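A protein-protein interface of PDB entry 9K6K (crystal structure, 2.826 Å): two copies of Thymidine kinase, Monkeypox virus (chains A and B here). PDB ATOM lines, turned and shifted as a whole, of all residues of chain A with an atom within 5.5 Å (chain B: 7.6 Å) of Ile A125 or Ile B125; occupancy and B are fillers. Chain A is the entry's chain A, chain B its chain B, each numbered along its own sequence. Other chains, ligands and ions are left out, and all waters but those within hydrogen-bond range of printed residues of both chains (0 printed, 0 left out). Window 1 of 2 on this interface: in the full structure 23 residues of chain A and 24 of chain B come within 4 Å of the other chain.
Printed residues of chain B within 4 Å of Asp A110: Ile B125 and Pro B126.
Of the printed residues of chain A, Ile B10 touches Ile A125 (3.7 Å).
Of chain A, only Ile A10 (3.7 Å), Asp A110 (3.4 Å), Leu A122 (3.7 Å), Ile A125 (3.5 Å) and Lys A133 (2.8 Å) come within 4 Å of Ile B125.
Of the printed residues of chain A, Phe B147 touches Pro A126 (3.7 Å) and Leu A127 (3.6 Å).
The nearest residue of chain B that does not touch Ile A125 is Leu B122 (4.6 Å).
Ile A10 touches Ile B125, and with the chains exchanged Ile A125 touches Ile B10.
Asp A110 touches Ile B125, and with the chains exchanged Ile A125 touches Asp B110.
Ile A125 touches Lys B133, and with the chains exchanged Lys A133 touches Ile B125.
Ser A128 touches Lys B133, and with the chains exchanged Lys A133 touches Ser B128.
Ile A10 touches Ile B125.
Asp A110 touches Pro B126.
O of Leu A122 touches CD1 of Leu B122 (3.2 Å).
Ile B125 touches Leu A122.
Asp B110 touches Ile A125.
Gly B111 touches Pro A126.
CB of Pro A126 touches O of Arg B115, 3.5 Å away.
CA of Pro B117 touches CG of Pro A126, 3.9 Å away.
Arg B115 touches Leu A127 (O to CD1, 3.3 Å).
Phe B147 touches Leu A127.
NZ of Lys A133 is in salt-bridge range of OD2 of Asp A110 (2.5 Å).
OG of Ser A128 lies within hydrogen-bond range of O of Leu A124 (2.6 Å).
OD2 of Asp B110 lies within salt-bridge range of NZ of Lys B133 (2.6 Å).
OG of Ser B128 lies within hydrogen-bond range of O of Leu B124, 2.5 Å away.
Of the 13 printed residues of chain A, 9 touch a printed residue of chain B.
Hydrophobic or aromatic side chains of chain A that line the printed part of chain B: Ile A10, Leu A122, Ile A125, Pro A126, Leu A127 and Val A131.
The backbone carbonyl oxygen (O) of Ile A125 is in hydrogen-bond range of the side-chain amino group (NZ) of Lys B133, at 3.2 Å.
The backbone carbonyl oxygen (O) of Ser A128 lies within hydrogen-bond range of the side-chain amino group (NZ) of Lys B133, 2.6 Å away.
N of Lys B133 is in hydrogen-bond range of O of Val A131, 3.4 Å away.
NZ of Lys A133 lies within hydrogen-bond range of O of Ile B125, at 2.8 Å.
NZ of Lys A133 sits at hydrogen-bond distance from O of Ser B128, at 2.7 Å.
N of Lys A133 sits at hydrogen-bond distance from O of Val B131.
The backbone carbonyl oxygen of Ile B125 sits close to the side-chain carboxylate of Asp A110 (3.4 Å).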
ATOM      1  N   LEU A   8      24.201 -16.599  22.013  1.00  0.00           N
ATOM      2  CA  LEU A   8      25.397 -15.818  22.283  1.00  0.00           C
ATOM      3  C   LEU A   8      25.386 -15.361  23.736  1.00  0.00           C
ATOM      4  O   LEU A   8      24.452 -14.671  24.168  1.00  0.00           O
ATOM      5  CB  LEU A   8      25.447 -14.610  21.338  1.00  0.00           C
ATOM      6  CG  LEU A   8      26.741 -14.196  20.638  1.00  0.00           C
ATOM      7  CD1 LEU A   8      27.553 -13.331  21.543  1.00  0.00           C
ATOM      8  CD2 LEU A   8      27.544 -15.420  20.220  1.00  0.00           C
ATOM      9  N   ILE A  10      27.687 -13.231  26.353  1.00  0.00           N
ATOM     10  CA  ILE A  10      28.836 -12.368  26.550  1.00  0.00           C
ATOM     11  C   ILE A  10      28.815 -11.844  27.978  1.00  0.00           C
ATOM     12  O   ILE A  10      27.891 -12.134  28.747  1.00  0.00           O
ATOM     13  CB  ILE A  10      28.821 -11.217  25.539  1.00  0.00           C
ATOM     14  CG1 ILE A  10      27.452 -10.533  25.564  1.00  0.00           C
ATOM     15  CG2 ILE A  10      29.091 -11.755  24.159  1.00  0.00           C
ATOM     16  CD1 ILE A  10      27.398  -9.211  24.804  1.00  0.00           C
ATOM     17  N   ASP A 110      32.997  -9.748  25.374  1.00  0.00           N
ATOM     18  CA  ASP A 110      32.554  -8.687  24.483  1.00  0.00           C
ATOM     19  C   ASP A 110      33.652  -7.650  24.279  1.00  0.00           C
ATOM     20  O   ASP A 110      33.802  -7.105  23.180  1.00  0.00           O
ATOM     21  CB  ASP A 110      31.296  -8.021  25.051  1.00  0.00           C
ATOM     22  CG  ASP A 110      31.487  -7.541  26.486  1.00  0.00           C
ATOM     23  OD1 ASP A 110      32.181  -8.225  27.267  1.00  0.00           O
ATOM     24  OD2 ASP A 110      30.960  -6.464  26.831  1.00  0.00           O
ATOM     25  N   ILE A 121      33.752 -11.388  17.356  1.00  0.00           N
ATOM     26  CA  ILE A 121      32.556 -11.734  18.122  1.00  0.00           C
ATOM     27  C   ILE A 121      31.395 -10.813  17.774  1.00  0.00           C
ATOM     28  O   ILE A 121      30.250 -11.263  17.644  1.00  0.00           O
ATOM     29  CB  ILE A 121      32.872 -11.702  19.629  1.00  0.00           C
ATOM     30  CG1 ILE A 121      33.654 -12.956  20.019  1.00  0.00           C
ATOM     31  CG2 ILE A 121      31.606 -11.499  20.458  1.00  0.00           C
ATOM     32  CD1 ILE A 121      32.980 -14.241  19.604  1.00  0.00           C
ATOM     33  N   LEU A 122      31.661  -9.512  17.627  1.00  0.00           N
ATOM     34  CA  LEU A 122      30.573  -8.576  17.360  1.00  0.00           C
ATOM     35  C   LEU A 122      29.910  -8.857  16.019  1.00  0.00           C
ATOM     36  O   LEU A 122      28.696  -8.676  15.878  1.00  0.00           O
ATOM     37  CB  LEU A 122      31.083  -7.136  17.415  1.00  0.00           C
ATOM     38  CG  LEU A 122      31.194  -6.514  18.809  1.00  0.00           C
ATOM     39  CD1 LEU A 122      29.932  -6.776  19.596  1.00  0.00           C
ATOM     40  CD2 LEU A 122      32.403  -7.021  19.575  1.00  0.00           C
ATOM     41  N   ASN A 123      30.678  -9.324  15.028  1.00  0.00           N
ATOM     42  CA  ASN A 123      30.082  -9.670  13.739  1.00  0.00           C
ATOM     43  C   ASN A 123      29.171 -10.883  13.806  1.00  0.00           C
ATOM     44  O   ASN A 123      28.558 -11.224  12.791  1.00  0.00           O
ATOM     45  CB  ASN A 123      31.168  -9.927  12.693  1.00  0.00           C
ATOM     46  CG  ASN A 123      32.019  -8.715  12.439  1.00  0.00           C
ATOM     47  OD1 ASN A 123      31.594  -7.588  12.686  1.00  0.00           O
ATOM     48  ND2 ASN A 123      33.223  -8.932  11.933  1.00  0.00           N
ATOM     49  N   LEU A 124      29.056 -11.533  14.959  1.00  0.00           N
ATOM     50  CA  LEU A 124      28.188 -12.689  15.098  1.00  0.00           C
ATOM     51  C   LEU A 124      26.796 -12.334  15.596  1.00  0.00           C
ATOM     52  O   LEU A 124      25.869 -13.135  15.430  1.00  0.00           O
ATOM     53  CB  LEU A 124      28.828 -13.694  16.056  1.00  0.00           C
ATOM     54  CG  LEU A 124      28.312 -15.124  16.059  1.00  0.00           C
ATOM     55  CD1 LEU A 124      28.404 -15.710  14.664  1.00  0.00           C
ATOM     56  CD2 LEU A 124      29.147 -15.923  17.036  1.00  0.00           C
ATOM     57  N   ILE A 125      26.619 -11.146  16.159  1.00  0.00           N
ATOM     58  CA  ILE A 125      25.355 -10.774  16.786  1.00  0.00           C
ATOM     59  C   ILE A 125      24.251 -10.547  15.756  1.00  0.00           C
ATOM     60  O   ILE A 125      23.141 -11.065  15.951  1.00  0.00           O
ATOM     61  CB  ILE A 125      25.547  -9.545  17.691  1.00  0.00           C
ATOM     62  CG1 ILE A 125      26.466  -9.900  18.864  1.00  0.00           C
ATOM     63  CG2 ILE A 125      24.211  -8.994  18.164  1.00  0.00           C
ATOM     64  CD1 ILE A 125      26.984  -8.706  19.625  1.00  0.00           C
ATOM     65  N   PRO A 126      24.472  -9.826  14.647  1.00  0.00           N
ATOM     66  CA  PRO A 126      23.413  -9.731  13.623  1.00  0.00           C
ATOM     67  C   PRO A 126      23.023 -11.071  13.006  1.00  0.00           C
ATOM     68  O   PRO A 126      22.042 -11.122  12.253  1.00  0.00           O
ATOM     69  CB  PRO A 126      24.016  -8.791  12.571  1.00  0.00           C
ATOM     70  CG  PRO A 126      25.015  -7.997  13.314  1.00  0.00           C
ATOM     71  CD  PRO A 126      25.603  -8.935  14.323  1.00  0.00           C
ATOM     72  N   LEU A 127      23.768 -12.145  13.283  1.00  0.00           N
ATOM     73  CA  LEU A 127      23.446 -13.474  12.787  1.00  0.00           C
ATOM     74  C   LEU A 127      22.884 -14.384  13.865  1.00  0.00           C
ATOM     75  O   LEU A 127      22.416 -15.484  13.541  1.00  0.00           O
ATOM     76  CB  LEU A 127      24.691 -14.140  12.168  1.00  0.00           C
ATOM     77  CG  LEU A 127      25.212 -13.649  10.809  1.00  0.00           C
ATOM     78  CD1 LEU A 127      25.750 -12.224  10.877  1.00  0.00           C
ATOM     79  CD2 LEU A 127      26.292 -14.556  10.295  1.00  0.00           C
ATOM     80  N   SER A 128      22.907 -13.959  15.124  1.00  0.00           N
ATOM     81  CA  SER A 128      22.506 -14.815  16.229  1.00  0.00           C
ATOM     82  C   SER A 128      21.026 -14.660  16.541  1.00  0.00           C
ATOM     83  O   SER A 128      20.442 -13.583  16.391  1.00  0.00           O
ATOM     84  CB  SER A 128      23.332 -14.511  17.479  1.00  0.00           C
ATOM     85  OG  SER A 128      24.716 -14.588  17.199  1.00  0.00           O
ATOM     86  N   VAL A 131      20.959 -13.248  22.204  1.00  0.00           N
ATOM     87  CA  VAL A 131      22.129 -12.549  22.732  1.00  0.00           C
ATOM     88  C   VAL A 131      21.837 -12.109  24.161  1.00  0.00           C
ATOM     89  O   VAL A 131      20.804 -11.489  24.424  1.00  0.00           O
ATOM     90  CB  VAL A 131      22.538 -11.347  21.862  1.00  0.00           C
ATOM     91  CG1 VAL A 131      23.690 -10.607  22.514  1.00  0.00           C
ATOM     92  CG2 VAL A 131      22.938 -11.815  20.463  1.00  0.00           C
ATOM     93  N   LYS A 133      23.949 -10.574  27.830  1.00  0.00           N
ATOM     94  CA  LYS A 133      25.164 -10.114  28.492  1.00  0.00           C
ATOM     95  C   LYS A 133      25.003 -10.309  29.993  1.00  0.00           C
ATOM     96  O   LYS A 133      24.061  -9.782  30.590  1.00  0.00           O
ATOM     97  CB  LYS A 133      25.479  -8.660  28.161  1.00  0.00           C
ATOM     98  CG  LYS A 133      26.750  -8.172  28.819  1.00  0.00           C
ATOM     99  CD  LYS A 133      27.299  -6.943  28.113  1.00  0.00           C
ATOM    100  CE  LYS A 133      28.616  -6.472  28.719  1.00  0.00           C
ATOM    101  NZ  LYS A 133      29.129  -5.265  28.002  1.00  0.00           N
ATOM    102  N   ILE B   6      24.778   2.169  30.741  1.00  0.00           N
ATOM    103  CA  ILE B   6      24.173   2.053  29.421  1.00  0.00           C
ATOM    104  C   ILE B   6      23.391   0.749  29.344  1.00  0.00           C
ATOM    105  O   ILE B   6      23.933  -0.338  29.603  1.00  0.00           O
ATOM    106  CB  ILE B   6      25.226   2.112  28.299  1.00  0.00           C
ATOM    107  CG1 ILE B   6      26.027   3.413  28.381  1.00  0.00           C
ATOM    108  CG2 ILE B   6      24.546   2.019  26.951  1.00  0.00           C
ATOM    109  CD1 ILE B   6      27.136   3.508  27.376  1.00  0.00           C
ATOM    110  N   LEU B   8      21.163  -1.488  26.655  1.00  0.00           N
ATOM    111  CA  LEU B   8      21.130  -1.705  25.218  1.00  0.00           C
ATOM    112  C   LEU B   8      20.056  -2.732  24.890  1.00  0.00           C
ATOM    113  O   LEU B   8      20.083  -3.859  25.404  1.00  0.00           O
ATOM    114  CB  LEU B   8      22.501  -2.195  24.731  1.00  0.00           C
ATOM    115  CG  LEU B   8      23.042  -1.740  23.377  1.00  0.00           C
ATOM    116  CD1 LEU B   8      22.351  -2.462  22.261  1.00  0.00           C
ATOM    117  CD2 LEU B   8      22.838  -0.252  23.244  1.00  0.00           C
ATOM    118  N   ILE B  10      18.444  -4.576  21.585  1.00  0.00           N
ATOM    119  CA  ILE B  10      18.473  -4.837  20.153  1.00  0.00           C
ATOM    120  C   ILE B  10      17.422  -5.887  19.831  1.00  0.00           C
ATOM    121  O   ILE B  10      16.728  -6.388  20.720  1.00  0.00           O
ATOM    122  CB  ILE B  10      19.855  -5.309  19.684  1.00  0.00           C
ATOM    123  CG1 ILE B  10      20.343  -6.457  20.579  1.00  0.00           C
ATOM    124  CG2 ILE B  10      20.830  -4.144  19.665  1.00  0.00           C
ATOM    125  CD1 ILE B  10      21.588  -7.194  20.055  1.00  0.00           C
ATOM    126  N   GLY B  11      17.342  -6.264  18.564  1.00  0.00           N
ATOM    127  CA  GLY B  11      16.318  -7.163  18.102  1.00  0.00           C
ATOM    128  C   GLY B  11      15.894  -6.797  16.702  1.00  0.00           C
ATOM    129  O   GLY B  11      16.297  -5.766  16.163  1.00  0.00           O
ATOM    130  N   VAL B  91      28.088   6.161  19.787  1.00  0.00           N
ATOM    131  CA  VAL B  91      28.950   5.558  20.799  1.00  0.00           C
ATOM    132  C   VAL B  91      29.588   6.626  21.681  1.00  0.00           C
ATOM    133  O   VAL B  91      29.530   6.544  22.915  1.00  0.00           O
ATOM    134  CB  VAL B  91      30.007   4.656  20.134  1.00  0.00           C
ATOM    135  CG1 VAL B  91      29.423   3.286  19.885  1.00  0.00           C
ATOM    136  CG2 VAL B  91      30.491   5.283  18.829  1.00  0.00           C
ATOM    137  N   ASP B 110      20.183  -4.554  15.440  1.00  0.00           N
ATOM    138  CA  ASP B 110      21.501  -5.172  15.424  1.00  0.00           C
ATOM    139  C   ASP B 110      21.988  -5.411  13.999  1.00  0.00           C
ATOM    140  O   ASP B 110      23.187  -5.285  13.720  1.00  0.00           O
ATOM    141  CB  ASP B 110      21.471  -6.480  16.211  1.00  0.00           C
ATOM    142  CG  ASP B 110      20.363  -7.406  15.751  1.00  0.00           C
ATOM    143  OD1 ASP B 110      19.279  -6.889  15.397  1.00  0.00           O
ATOM    144  OD2 ASP B 110      20.571  -8.640  15.749  1.00  0.00           O
ATOM    145  N   GLY B 111      21.085  -5.755  13.088  1.00  0.00           N
ATOM    146  CA  GLY B 111      21.473  -6.070  11.726  1.00  0.00           C
ATOM    147  C   GLY B 111      20.548  -5.440  10.706  1.00  0.00           C
ATOM    148  O   GLY B 111      19.353  -5.247  10.946  1.00  0.00           O
ATOM    149  N   ARG B 115      21.481  -8.839   7.173  1.00  0.00           N
ATOM    150  CA  ARG B 115      22.016  -9.424   8.404  1.00  0.00           C
ATOM    151  C   ARG B 115      23.474  -9.036   8.635  1.00  0.00           C
ATOM    152  O   ARG B 115      24.253  -9.804   9.204  1.00  0.00           O
ATOM    153  CB  ARG B 115      21.862 -10.945   8.404  1.00  0.00           C
ATOM    154  CG  ARG B 115      20.431 -11.417   8.401  1.00  0.00           C
ATOM    155  CD  ARG B 115      20.354 -12.825   8.927  1.00  0.00           C
ATOM    156  NE  ARG B 115      21.029 -13.787   8.057  1.00  0.00           N
ATOM    157  CZ  ARG B 115      21.409 -14.995   8.453  1.00  0.00           C
ATOM    158  NH1 ARG B 115      21.193 -15.372   9.705  1.00  0.00           N
ATOM    159  NH2 ARG B 115      22.010 -15.817   7.607  1.00  0.00           N
ATOM    160  N   PRO B 117      26.195  -5.913  10.137  1.00  0.00           N
ATOM    161  CA  PRO B 117      26.113  -4.943  11.241  1.00  0.00           C
ATOM    162  C   PRO B 117      25.641  -3.585  10.746  1.00  0.00           C
ATOM    163  O   PRO B 117      25.980  -3.148   9.645  1.00  0.00           O
ATOM    164  CB  PRO B 117      27.552  -4.887  11.770  1.00  0.00           C
ATOM    165  CG  PRO B 117      28.401  -5.385  10.638  1.00  0.00           C
ATOM    166  CD  PRO B 117      27.565  -6.420   9.945  1.00  0.00           C
ATOM    167  N   ASN B 120      27.496   2.063  13.319  1.00  0.00           N
ATOM    168  CA  ASN B 120      28.440   1.979  14.426  1.00  0.00           C
ATOM    169  C   ASN B 120      27.719   1.651  15.730  1.00  0.00           C
ATOM    170  O   ASN B 120      28.013   2.216  16.786  1.00  0.00           O
ATOM    171  CB  ASN B 120      29.231   3.283  14.560  1.00  0.00           C
ATOM    172  CG  ASN B 120      30.611   3.081  15.176  1.00  0.00           C
ATOM    173  OD1 ASN B 120      30.765   3.058  16.398  1.00  0.00           O
ATOM    174  ND2 ASN B 120      31.624   2.955  14.325  1.00  0.00           N
ATOM    175  N   ILE B 121      26.756   0.729  15.671  1.00  0.00           N
ATOM    176  CA  ILE B 121      25.970   0.394  16.854  1.00  0.00           C
ATOM    177  C   ILE B 121      26.559  -0.760  17.667  1.00  0.00           C
ATOM    178  O   ILE B 121      26.251  -0.881  18.861  1.00  0.00           O
ATOM    179  CB  ILE B 121      24.514   0.080  16.461  1.00  0.00           C
ATOM    180  CG1 ILE B 121      23.593   0.206  17.676  1.00  0.00           C
ATOM    181  CG2 ILE B 121      24.393  -1.316  15.866  1.00  0.00           C
ATOM    182  CD1 ILE B 121      23.630   1.569  18.321  1.00  0.00           C
ATOM    183  N   LEU B 122      27.407  -1.601  17.066  1.00  0.00           N
ATOM    184  CA  LEU B 122      27.965  -2.729  17.803  1.00  0.00           C
ATOM    185  C   LEU B 122      29.119  -2.306  18.706  1.00  0.00           C
ATOM    186  O   LEU B 122      29.313  -2.885  19.781  1.00  0.00           O
ATOM    187  CB  LEU B 122      28.413  -3.818  16.833  1.00  0.00           C
ATOM    188  CG  LEU B 122      27.245  -4.488  16.114  1.00  0.00           C
ATOM    189  CD1 LEU B 122      27.708  -5.676  15.304  1.00  0.00           C
ATOM    190  CD2 LEU B 122      26.161  -4.890  17.114  1.00  0.00           C
ATOM    191  N   ASN B 123      29.876  -1.283  18.312  1.00  0.00           N
ATOM    192  CA  ASN B 123      30.964  -0.750  19.130  1.00  0.00           C
ATOM    193  C   ASN B 123      30.484  -0.215  20.477  1.00  0.00           C
ATOM    194  O   ASN B 123      31.292   0.232  21.295  1.00  0.00           O
ATOM    195  CB  ASN B 123      31.710   0.347  18.362  1.00  0.00           C
ATOM    196  CG  ASN B 123      32.388  -0.176  17.111  1.00  0.00           C
ATOM    197  OD1 ASN B 123      32.704  -1.360  17.019  1.00  0.00           O
ATOM    198  ND2 ASN B 123      32.608   0.701  16.141  1.00  0.00           N
ATOM    199  N   LEU B 124      29.175  -0.263  20.720  1.00  0.00           N
ATOM    200  CA  LEU B 124      28.595   0.206  21.969  1.00  0.00           C
ATOM    201  C   LEU B 124      28.477  -0.897  23.009  1.00  0.00           C
ATOM    202  O   LEU B 124      28.294  -0.596  24.195  1.00  0.00           O
ATOM    203  CB  LEU B 124      27.214   0.811  21.693  1.00  0.00           C
ATOM    204  CG  LEU B 124      26.554   1.724  22.720  1.00  0.00           C
ATOM    205  CD1 LEU B 124      27.478   2.877  23.041  1.00  0.00           C
ATOM    206  CD2 LEU B 124      25.241   2.248  22.159  1.00  0.00           C
ATOM    207  N   ILE B 125      28.597  -2.155  22.599  1.00  0.00           N
ATOM    208  CA  ILE B 125      28.398  -3.294  23.496  1.00  0.00           C
ATOM    209  C   ILE B 125      29.554  -3.435  24.485  1.00  0.00           C
ATOM    210  O   ILE B 125      29.305  -3.693  25.674  1.00  0.00           O
ATOM    211  CB  ILE B 125      28.186  -4.573  22.678  1.00  0.00           C
ATOM    212  CG1 ILE B 125      26.904  -4.413  21.865  1.00  0.00           C
ATOM    213  CG2 ILE B 125      28.120  -5.783  23.588  1.00  0.00           C
ATOM    214  CD1 ILE B 125      26.758  -5.394  20.755  1.00  0.00           C
ATOM    215  N   PRO B 126      30.820  -3.297  24.066  1.00  0.00           N
ATOM    216  CA  PRO B 126      31.913  -3.272  25.055  1.00  0.00           C
ATOM    217  C   PRO B 126      31.822  -2.119  26.032  1.00  0.00           C
ATOM    218  O   PRO B 126      32.553  -2.118  27.027  1.00  0.00           O
ATOM    219  CB  PRO B 126      33.170  -3.140  24.188  1.00  0.00           C
ATOM    220  CG  PRO B 126      32.771  -3.690  22.880  1.00  0.00           C
ATOM    221  CD  PRO B 126      31.351  -3.306  22.692  1.00  0.00           C
ATOM    222  N   LEU B 127      30.954  -1.146  25.789  1.00  0.00           N
ATOM    223  CA  LEU B 127      30.789  -0.016  26.684  1.00  0.00           C
ATOM    224  C   LEU B 127      29.506  -0.081  27.499  1.00  0.00           C
ATOM    225  O   LEU B 127      29.342   0.720  28.425  1.00  0.00           O
ATOM    226  CB  LEU B 127      30.817   1.291  25.878  1.00  0.00           C
ATOM    227  CG  LEU B 127      32.149   1.789  25.295  1.00  0.00           C
ATOM    228  CD1 LEU B 127      32.708   0.885  24.209  1.00  0.00           C
ATOM    229  CD2 LEU B 127      31.969   3.201  24.751  1.00  0.00           C
ATOM    230  N   SER B 128      28.612  -1.020  27.200  1.00  0.00           N
ATOM    231  CA  SER B 128      27.314  -1.094  27.854  1.00  0.00           C
ATOM    232  C   SER B 128      27.353  -2.001  29.080  1.00  0.00           C
ATOM    233  O   SER B 128      28.030  -3.033  29.099  1.00  0.00           O
ATOM    234  CB  SER B 128      26.258  -1.612  26.877  1.00  0.00           C
ATOM    235  OG  SER B 128      26.268  -0.854  25.680  1.00  0.00           O
ATOM    236  N   GLU B 129      26.568  -1.627  30.094  1.00  0.00           N
ATOM    237  CA  GLU B 129      26.460  -2.466  31.279  1.00  0.00           C
ATOM    238  C   GLU B 129      25.440  -3.569  31.084  1.00  0.00           C
ATOM    239  O   GLU B 129      25.627  -4.673  31.614  1.00  0.00           O
ATOM    240  CB  GLU B 129      26.081  -1.629  32.504  1.00  0.00           C
ATOM    241  CG  GLU B 129      27.238  -0.945  33.215  1.00  0.00           C
ATOM    242  CD  GLU B 129      27.674   0.350  32.552  1.00  0.00           C
ATOM    243  OE1 GLU B 129      27.276   0.600  31.394  1.00  0.00           O
ATOM    244  OE2 GLU B 129      28.396   1.135  33.210  1.00  0.00           O
ATOM    245  N   MET B 130      24.371  -3.307  30.329  1.00  0.00           N
ATOM    246  CA  MET B 130      23.409  -4.369  30.066  1.00  0.00           C
ATOM    247  C   MET B 130      23.060  -4.401  28.589  1.00  0.00           C
ATOM    248  O   MET B 130      22.834  -3.352  27.979  1.00  0.00           O
ATOM    249  CB  MET B 130      22.145  -4.231  30.916  1.00  0.00           C
ATOM    250  CG  MET B 130      21.825  -2.858  31.367  1.00  0.00           C
ATOM    251  SD  MET B 130      20.775  -2.983  32.822  1.00  0.00           S
ATOM    252  CE  MET B 130      21.952  -3.664  33.992  1.00  0.00           C
ATOM    253  N   VAL B 131      23.027  -5.609  28.021  1.00  0.00           N
ATOM    254  CA  VAL B 131      22.700  -5.828  26.618  1.00  0.00           C
ATOM    255  C   VAL B 131      21.696  -6.966  26.533  1.00  0.00           C
ATOM    256  O   VAL B 131      21.934  -8.039  27.092  1.00  0.00           O
ATOM    257  CB  VAL B 131      23.954  -6.169  25.792  1.00  0.00           C
ATOM    258  CG1 VAL B 131      23.575  -6.464  24.350  1.00  0.00           C
ATOM    259  CG2 VAL B 131      24.979  -5.052  25.868  1.00  0.00           C
ATOM    260  N   LYS B 133      18.786  -8.921  23.662  1.00  0.00           N
ATOM    261  CA  LYS B 133      18.230  -9.062  22.326  1.00  0.00           C
ATOM    262  C   LYS B 133      16.808  -9.598  22.429  1.00  0.00           C
ATOM    263  O   LYS B 133      16.584 -10.685  22.973  1.00  0.00           O
ATOM    264  CB  LYS B 133      19.085  -9.977  21.454  1.00  0.00           C
ATOM    265  CG  LYS B 133      18.515 -10.110  20.061  1.00  0.00           C
ATOM    266  CD  LYS B 133      19.560 -10.543  19.074  1.00  0.00           C
ATOM    267  CE  LYS B 133      19.001 -10.556  17.664  1.00  0.00           C
ATOM    268  NZ  LYS B 133      20.059 -10.991  16.695  1.00  0.00           N
ATOM    269  N   SER B 146      14.194 -13.479  14.385  1.00  0.00           N
ATOM    270  CA  SER B 146      15.324 -12.694  14.857  1.00  0.00           C
ATOM    271  C   SER B 146      15.972 -11.896  13.740  1.00  0.00           C
ATOM    272  O   SER B 146      17.034 -11.299  13.959  1.00  0.00           O
ATOM    273  CB  SER B 146      16.373 -13.569  15.547  1.00  0.00           C
ATOM    274  OG  SER B 146      15.865 -14.071  16.769  1.00  0.00           O
ATOM    275  N   PHE B 147      15.380 -11.876  12.548  1.00  0.00           N
ATOM    276  CA  PHE B 147      15.974 -11.139  11.448  1.00  0.00           C
ATOM    277  C   PHE B 147      14.891 -10.337  10.747  1.00  0.00           C
ATOM    278  O   PHE B 147      13.696 -10.591  10.914  1.00  0.00           O
ATOM    279  CB  PHE B 147      16.695 -12.078  10.473  1.00  0.00           C
ATOM    280  CG  PHE B 147      17.517 -13.137  11.157  1.00  0.00           C
ATOM    281  CD1 PHE B 147      18.688 -12.800  11.819  1.00  0.00           C
ATOM    282  CD2 PHE B 147      17.126 -14.465  11.128  1.00  0.00           C
ATOM    283  CE1 PHE B 147      19.449 -13.764  12.445  1.00  0.00           C
ATOM    284  CE2 PHE B 147      17.886 -15.435  11.753  1.00  0.00           C
ATOM    285  CZ  PHE B 147      19.049 -15.082  12.414  1.00  0.00           C
